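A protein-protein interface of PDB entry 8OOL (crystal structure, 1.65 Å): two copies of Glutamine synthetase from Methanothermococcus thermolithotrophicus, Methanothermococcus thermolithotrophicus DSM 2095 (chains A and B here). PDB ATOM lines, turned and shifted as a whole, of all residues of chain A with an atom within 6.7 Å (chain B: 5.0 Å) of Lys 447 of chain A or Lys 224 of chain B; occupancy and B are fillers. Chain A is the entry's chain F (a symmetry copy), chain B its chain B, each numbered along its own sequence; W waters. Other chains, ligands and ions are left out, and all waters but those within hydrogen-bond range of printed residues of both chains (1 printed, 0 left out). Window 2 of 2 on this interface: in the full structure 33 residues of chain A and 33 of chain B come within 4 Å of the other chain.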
ATOM      1  N   THR A 442     -19.910  -0.550  13.883  1.00  0.00           N
ATOM      2  CA  THR A 442     -19.871  -2.030  13.771  1.00  0.00           C
ATOM      3  C   THR A 442     -20.965  -2.615  14.671  1.00  0.00           C
ATOM      4  O   THR A 442     -21.686  -3.515  14.225  1.00  0.00           O
ATOM      5  CB  THR A 442     -18.467  -2.567  14.080  1.00  0.00           C
ATOM      6  OG1 THR A 442     -17.588  -2.090  13.062  1.00  0.00           O
ATOM      7  CG2 THR A 442     -18.411  -4.077  14.152  1.00  0.00           C
ATOM      8  N   THR A 443     -21.075  -2.090  15.890  1.00  0.00           N
ATOM      9  CA  THR A 443     -22.096  -2.600  16.841  1.00  0.00           C
ATOM     10  C   THR A 443     -23.497  -2.331  16.283  1.00  0.00           C
ATOM     11  O   THR A 443     -24.358  -3.206  16.412  1.00  0.00           O
ATOM     12  CB  THR A 443     -21.880  -1.985  18.233  1.00  0.00           C
ATOM     13  OG1 THR A 443     -20.619  -2.422  18.738  1.00  0.00           O
ATOM     14  CG2 THR A 443     -22.979  -2.342  19.209  1.00  0.00           C
ATOM     15  N   ALA A 444     -23.692  -1.176  15.649  1.00  0.00           N
ATOM     16  CA  ALA A 444     -25.041  -0.789  15.181  1.00  0.00           C
ATOM     17  C   ALA A 444     -25.427  -1.408  13.836  1.00  0.00           C
ATOM     18  O   ALA A 444     -26.626  -1.671  13.656  1.00  0.00           O
ATOM     19  CB  ALA A 444     -25.092   0.712  15.061  1.00  0.00           C
ATOM     20  N   TYR A 445     -24.464  -1.666  12.950  1.00  0.00           N
ATOM     21  CA  TYR A 445     -24.855  -2.041  11.563  1.00  0.00           C
ATOM     22  C   TYR A 445     -24.350  -3.398  11.052  1.00  0.00           C
ATOM     23  O   TYR A 445     -24.795  -3.790   9.969  1.00  0.00           O
ATOM     24  CB  TYR A 445     -24.377  -0.928  10.624  1.00  0.00           C
ATOM     25  CG  TYR A 445     -24.857   0.449  11.001  1.00  0.00           C
ATOM     26  CD1 TYR A 445     -26.207   0.722  11.132  1.00  0.00           C
ATOM     27  CD2 TYR A 445     -23.962   1.481  11.232  1.00  0.00           C
ATOM     28  CE1 TYR A 445     -26.659   1.984  11.477  1.00  0.00           C
ATOM     29  CE2 TYR A 445     -24.398   2.749  11.575  1.00  0.00           C
ATOM     30  CZ  TYR A 445     -25.750   3.003  11.700  1.00  0.00           C
ATOM     31  OH  TYR A 445     -26.187   4.257  12.041  1.00  0.00           O
ATOM     32  N   LEU A 446     -23.478  -4.095  11.773  1.00  0.00           N
ATOM     33  CA  LEU A 446     -22.969  -5.362  11.179  1.00  0.00           C
ATOM     34  C   LEU A 446     -24.148  -6.307  10.902  1.00  0.00           C
ATOM     35  O   LEU A 446     -24.052  -7.097   9.955  1.00  0.00           O
ATOM     36  CB  LEU A 446     -21.928  -5.999  12.103  1.00  0.00           C
ATOM     37  CG  LEU A 446     -20.916  -6.903  11.403  1.00  0.00           C
ATOM     38  CD1 LEU A 446     -20.129  -6.125  10.361  1.00  0.00           C
ATOM     39  CD2 LEU A 446     -19.977  -7.548  12.411  1.00  0.00           C
ATOM     40  N   LYS A 447     -25.226  -6.194  11.673  1.00  0.00           N
ATOM     41  CA  LYS A 447     -26.395  -7.104  11.525  1.00  0.00           C
ATOM     42  C   LYS A 447     -27.288  -6.740  10.332  1.00  0.00           C
ATOM     43  O   LYS A 447     -28.147  -7.568   9.994  1.00  0.00           O
ATOM     44  CB  LYS A 447     -27.263  -7.058  12.785  1.00  0.00           C
ATOM     45  CG  LYS A 447     -28.094  -5.792  12.941  1.00  0.00           C
ATOM     46  CD  LYS A 447     -28.546  -5.532  14.362  1.00  0.00           C
ATOM     47  CE  LYS A 447     -29.146  -4.156  14.546  1.00  0.00           C
ATOM     48  NZ  LYS A 447     -30.207  -4.153  15.579  1.00  0.00           N
ATOM     49  N   ILE A 448     -27.136  -5.558   9.735  1.00  0.00           N
ATOM     50  CA  ILE A 448     -28.064  -5.193   8.663  1.00  0.00           C
ATOM     51  C   ILE A 448     -27.861  -5.959   7.336  1.00  0.00           C
ATOM     52  O   ILE A 448     -26.754  -6.543   7.146  1.00  0.00           O
ATOM     53  CB  ILE A 448     -28.079  -3.668   8.465  1.00  0.00           C
ATOM     54  CG1 ILE A 448     -26.793  -3.169   7.772  1.00  0.00           C
ATOM     55  CG2 ILE A 448     -28.341  -2.959   9.810  1.00  0.00           C
ATOM     56  CD1 ILE A 448     -26.609  -1.631   7.801  1.00  0.00           C
ATOM     57  OXT ILE A 448     -28.838  -5.973   6.521  1.00  0.00           O
ATOM     58  N   PHE B 219     -33.928 -11.310  -1.036  1.00  0.00           N
ATOM     59  CA  PHE B 219     -32.517 -11.646  -1.173  1.00  0.00           C
ATOM     60  C   PHE B 219     -31.758 -11.393   0.139  1.00  0.00           C
ATOM     61  O   PHE B 219     -30.942 -12.212   0.515  1.00  0.00           O
ATOM     62  CB  PHE B 219     -31.940 -10.740  -2.283  1.00  0.00           C
ATOM     63  CG  PHE B 219     -30.445 -10.538  -2.248  1.00  0.00           C
ATOM     64  CD1 PHE B 219     -29.582 -11.600  -2.456  1.00  0.00           C
ATOM     65  CD2 PHE B 219     -29.911  -9.269  -2.071  1.00  0.00           C
ATOM     66  CE1 PHE B 219     -28.191 -11.406  -2.434  1.00  0.00           C
ATOM     67  CE2 PHE B 219     -28.531  -9.069  -2.079  1.00  0.00           C
ATOM     68  CZ  PHE B 219     -27.687 -10.132  -2.265  1.00  0.00           C
ATOM     69  N   LYS B 220     -32.013 -10.266   0.815  1.00  0.00           N
ATOM     70  CA  LYS B 220     -31.257  -9.982   2.043  1.00  0.00           C
ATOM     71  C   LYS B 220     -31.469 -11.077   3.104  1.00  0.00           C
ATOM     72  O   LYS B 220     -30.507 -11.547   3.713  1.00  0.00           O
ATOM     73  CB  LYS B 220     -31.592  -8.564   2.557  1.00  0.00           C
ATOM     74  CG  LYS B 220     -31.143  -7.487   1.558  1.00  0.00           C
ATOM     75  CD  LYS B 220     -31.694  -6.113   1.900  1.00  0.00           C
ATOM     76  CE  LYS B 220     -30.901  -5.402   2.949  1.00  0.00           C
ATOM     77  NZ  LYS B 220     -31.472  -4.038   3.231  1.00  0.00           N
ATOM     78  N   THR B 221     -32.709 -11.540   3.295  1.00  0.00           N
ATOM     79  CA  THR B 221     -32.901 -12.613   4.269  1.00  0.00           C
ATOM     80  C   THR B 221     -32.227 -13.898   3.802  1.00  0.00           C
ATOM     81  O   THR B 221     -31.542 -14.597   4.563  1.00  0.00           O
ATOM     82  CB  THR B 221     -34.422 -12.901   4.428  1.00  0.00           C
ATOM     83  OG1 THR B 221     -35.044 -11.733   4.963  1.00  0.00           O
ATOM     84  CG2 THR B 221     -34.685 -14.099   5.389  1.00  0.00           C
ATOM     85  N   THR B 222     -32.441 -14.218   2.527  1.00  0.00           N
ATOM     86  CA  THR B 222     -31.932 -15.485   1.984  1.00  0.00           C
ATOM     87  C   THR B 222     -30.416 -15.587   2.015  1.00  0.00           C
ATOM     88  O   THR B 222     -29.892 -16.646   2.400  1.00  0.00           O
ATOM     89  CB  THR B 222     -32.537 -15.735   0.580  1.00  0.00           C
ATOM     90  OG1 THR B 222     -33.977 -15.585   0.626  1.00  0.00           O
ATOM     91  CG2 THR B 222     -32.236 -17.183   0.108  1.00  0.00           C
ATOM     92  N   ILE B 223     -29.691 -14.525   1.623  1.00  0.00           N
ATOM     93  CA  ILE B 223     -28.217 -14.638   1.659  1.00  0.00           C
ATOM     94  C   ILE B 223     -27.719 -14.787   3.096  1.00  0.00           C
ATOM     95  O   ILE B 223     -26.745 -15.497   3.330  1.00  0.00           O
ATOM     96  CB  ILE B 223     -27.541 -13.451   0.894  1.00  0.00           C
ATOM     97  CG1 ILE B 223     -26.020 -13.688   0.769  1.00  0.00           C
ATOM     98  CG2 ILE B 223     -27.815 -12.152   1.591  1.00  0.00           C
ATOM     99  CD1 ILE B 223     -25.634 -14.974  -0.018  1.00  0.00           C
ATOM    100  N   LYS B 224     -28.405 -14.150   4.063  1.00  0.00           N
ATOM    101  CA  LYS B 224     -27.965 -14.263   5.461  1.00  0.00           C
ATOM    102  C   LYS B 224     -28.171 -15.705   5.926  1.00  0.00           C
ATOM    103  O   LYS B 224     -27.326 -16.243   6.632  1.00  0.00           O
ATOM    104  CB  LYS B 224     -28.746 -13.289   6.342  1.00  0.00           C
ATOM    105  CG  LYS B 224     -28.356 -11.849   6.093  1.00  0.00           C
ATOM    106  CD  LYS B 224     -29.251 -10.911   6.877  1.00  0.00           C
ATOM    107  CE  LYS B 224     -28.787  -9.484   6.716  1.00  0.00           C
ATOM    108  NZ  LYS B 224     -27.521  -9.279   7.502  1.00  0.00           N
ATOM    109  N   THR B 225     -29.284 -16.344   5.542  1.00  0.00           N
ATOM    110  CA  THR B 225     -29.471 -17.746   5.961  1.00  0.00           C
ATOM    111  C   THR B 225     -28.528 -18.696   5.246  1.00  0.00           C
ATOM    112  O   THR B 225     -28.039 -19.639   5.871  1.00  0.00           O
ATOM    113  CB  THR B 225     -30.942 -18.206   5.791  1.00  0.00           C
ATOM    114  OG1 THR B 225     -31.252 -18.251   4.389  1.00  0.00           O
ATOM    115  CG2 THR B 225     -31.893 -17.272   6.459  1.00  0.00           C
ATOM    116  N   ILE B 226     -28.264 -18.481   3.966  1.00  0.00           N
ATOM    117  CA  ILE B 226     -27.324 -19.359   3.254  1.00  0.00           C
ATOM    118  C   ILE B 226     -25.937 -19.158   3.908  1.00  0.00           C
ATOM    119  O   ILE B 226     -25.254 -20.155   4.185  1.00  0.00           O
ATOM    120  CB  ILE B 226     -27.342 -19.024   1.741  1.00  0.00           C
ATOM    121  CG1 ILE B 226     -28.652 -19.547   1.120  1.00  0.00           C
ATOM    122  CG2 ILE B 226     -26.089 -19.594   1.024  1.00  0.00           C
ATOM    123  CD1 ILE B 226     -28.882 -19.106  -0.397  1.00  0.00           C
ATOM    124  N   ALA B 227     -25.521 -17.888   4.173  1.00  0.00           N
ATOM    125  CA  ALA B 227     -24.209 -17.654   4.810  1.00  0.00           C
ATOM    126  C   ALA B 227     -24.099 -18.424   6.149  1.00  0.00           C
ATOM    127  O   ALA B 227     -23.095 -19.072   6.395  1.00  0.00           O
ATOM    128  CB  ALA B 227     -24.000 -16.167   5.077  1.00  0.00           C
ATOM    129  N   GLU B 228     -25.131 -18.364   6.993  1.00  0.00           N
ATOM    130  CA  GLU B 228     -25.099 -19.069   8.280  1.00  0.00           C
ATOM    131  C   GLU B 228     -24.938 -20.589   8.123  1.00  0.00           C
ATOM    132  O   GLU B 228     -24.224 -21.218   8.931  1.00  0.00           O
ATOM    133  CB  GLU B 228     -26.366 -18.772   9.074  1.00  0.00           C
ATOM    134  CG  GLU B 228     -26.311 -17.392   9.676  1.00  0.00           C
ATOM    135  CD  GLU B 228     -27.088 -17.249  10.965  1.00  0.00           C
ATOM    136  OE1 GLU B 228     -27.932 -18.128  11.266  1.00  0.00           O
ATOM    137  OE2 GLU B 228     -26.851 -16.244  11.672  1.00  0.00           O
ATOM    138  N   LYS B 233     -21.260 -15.052   8.117  1.00  0.00           N
ATOM    139  CA  LYS B 233     -22.288 -14.014   8.361  1.00  0.00           C
ATOM    140  C   LYS B 233     -22.317 -13.103   7.133  1.00  0.00           C
ATOM    141  O   LYS B 233     -21.232 -12.757   6.666  1.00  0.00           O
ATOM    142  CB  LYS B 233     -21.929 -13.200   9.606  1.00  0.00           C
ATOM    143  CG  LYS B 233     -22.976 -12.175  10.011  1.00  0.00           C
ATOM    144  CD  LYS B 233     -22.567 -11.290  11.164  1.00  0.00           C
ATOM    145  CE  LYS B 233     -23.380 -10.016  11.220  1.00  0.00           C
ATOM    146  NZ  LYS B 233     -24.269  -9.874  10.042  1.00  0.00           N
ATOM    147  N   ALA B 234     -23.498 -12.760   6.610  1.00  0.00           N
ATOM    148  CA  ALA B 234     -23.509 -11.844   5.446  1.00  0.00           C
ATOM    149  C   ALA B 234     -23.918 -10.479   6.023  1.00  0.00           C
ATOM    150  O   ALA B 234     -24.816 -10.425   6.890  1.00  0.00           O
ATOM    151  CB  ALA B 234     -24.552 -12.275   4.404  1.00  0.00           C
ATOM    152  N   THR B 235     -23.253  -9.414   5.565  1.00  0.00           N
ATOM    153  CA  THR B 235     -23.582  -8.050   6.056  1.00  0.00           C
ATOM    154  C   THR B 235     -23.807  -7.058   4.910  1.00  0.00           C
ATOM    155  O   THR B 235     -23.069  -7.117   3.920  1.00  0.00           O
ATOM    156  CB  THR B 235     -22.502  -7.474   6.984  1.00  0.00           C
ATOM    157  OG1 THR B 235     -23.011  -6.256   7.528  1.00  0.00           O
ATOM    158  CG2 THR B 235     -21.187  -7.216   6.282  1.00  0.00           C
ATOM    159  N   PHE B 236     -24.796  -6.177   5.078  1.00  0.00           N
ATOM    160  CA  PHE B 236     -25.049  -5.112   4.077  1.00  0.00           C
ATOM    161  C   PHE B 236     -24.566  -3.785   4.674  1.00  0.00           C
ATOM    162  O   PHE B 236     -24.923  -2.722   4.152  1.00  0.00           O
ATOM    163  CB  PHE B 236     -26.522  -5.114   3.663  1.00  0.00           C
ATOM    164  CG  PHE B 236     -26.921  -6.328   2.866  1.00  0.00           C
ATOM    165  CD1 PHE B 236     -26.607  -6.428   1.521  1.00  0.00           C
ATOM    166  CD2 PHE B 236     -27.587  -7.383   3.467  1.00  0.00           C
ATOM    167  CE1 PHE B 236     -26.965  -7.549   0.791  1.00  0.00           C
ATOM    168  CE2 PHE B 236     -27.944  -8.504   2.735  1.00  0.00           C
ATOM    169  CZ  PHE B 236     -27.633  -8.584   1.399  1.00  0.00           C
HETATM  170  O   HOH W   1     -29.772  -3.670   5.377  1.00  0.00           O
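NZ of Lys 224 of chain B lies within hydrogen-bond range of O of Ala 234 of chain B (3.0 Å).
No position is printed for both chains.
Of the 8 pairs that touch across the chains among the printed residues, none has its exchanged pair printed and touching as well.
Thr 443 of chain A touches none of the printed residues of chain B.
Of the printed residues of chain B, Tyr 445 of chain A touches Thr 235.
Lys 447 of chain A touches just these residues of chain B: Lys 224 (3.1 Å) and Lys 233 (3.8 Å).
Lys 220 of chain B touches none of the printed residues of chain A.
Of chain A, only Lys 447 and Ile 448 come within 4 Å of Lys 224 of chain B.
Of the printed residues of chain A, Lys 233 of chain B touches Leu 446 (2.8 Å) and Lys 447 (3.8 Å).
Printed residues of chain A within 4 Å of Thr 235 of chain B: Tyr 445, Leu 446 and Ile 448.
Printed residues of chain A within 4 Å of Phe 236 of chain B: Ile 448 (2.9 Å).
The nearest residue of chain B that does not touch Lys 447 of chain A is Thr 235 of chain B (4.7 Å).
O of Tyr 445 of chain A touches OG1 of Thr 235 of chain B, at 3.9 Å.
CA of Lys 447 of chain A touches NZ of Lys 233 of chain B (3.8 Å).
O of Ile 448 of chain A touches CA of Thr 235 of chain B, at 3.7 Å.
N of Phe 236 of chain B sits at hydrogen-bond distance from O of Ile 448 of chain A (2.9 Å).
The backbone carbonyl oxygen (O) of Leu 446 of chain A sits at hydrogen-bond distance from the side-chain amino group (NZ) of Lys 233 of chain B (2.8 Å).
OG1 of Thr 235 of chain B lies within hydrogen-bond range of O of Leu 446 of chain A (2.8 Å).
O of Lys 447 of chain A lies within hydrogen-bond range of NZ of Lys 224 of chain B, 3.1 Å away.
The side-chain amino group (NZ) of Lys 224 of chain B lies within salt-bridge range of the chain-end carboxylate (O) of Ile 448 of chain A, at 2.9 Å.
Printed residues of chain B that touch a printed residue of chain A: Lys 224, Lys 233, Thr 235 and Phe 236.
Of the 7 printed residues of chain A, 4 touch a printed residue of chain B.
Printed residues of chain A that touch a printed residue of chain B: Tyr 445, Leu 446, Lys 447 and Ile 448.
Hydrophobic or aromatic side chains of chain A within 4 Å of the printed part of chain B: Leu 446 and Ile 448.
Among the printed residues, no Asp or Glu carboxylate lies within 4 Å of a Lys or Arg side-chain nitrogen of the other chain.
Water W1 bridges the chain-end carboxylate (OXT) of Ile 448 of chain A and the side-chain amino group (NZ) of Lys 220 of chain B.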
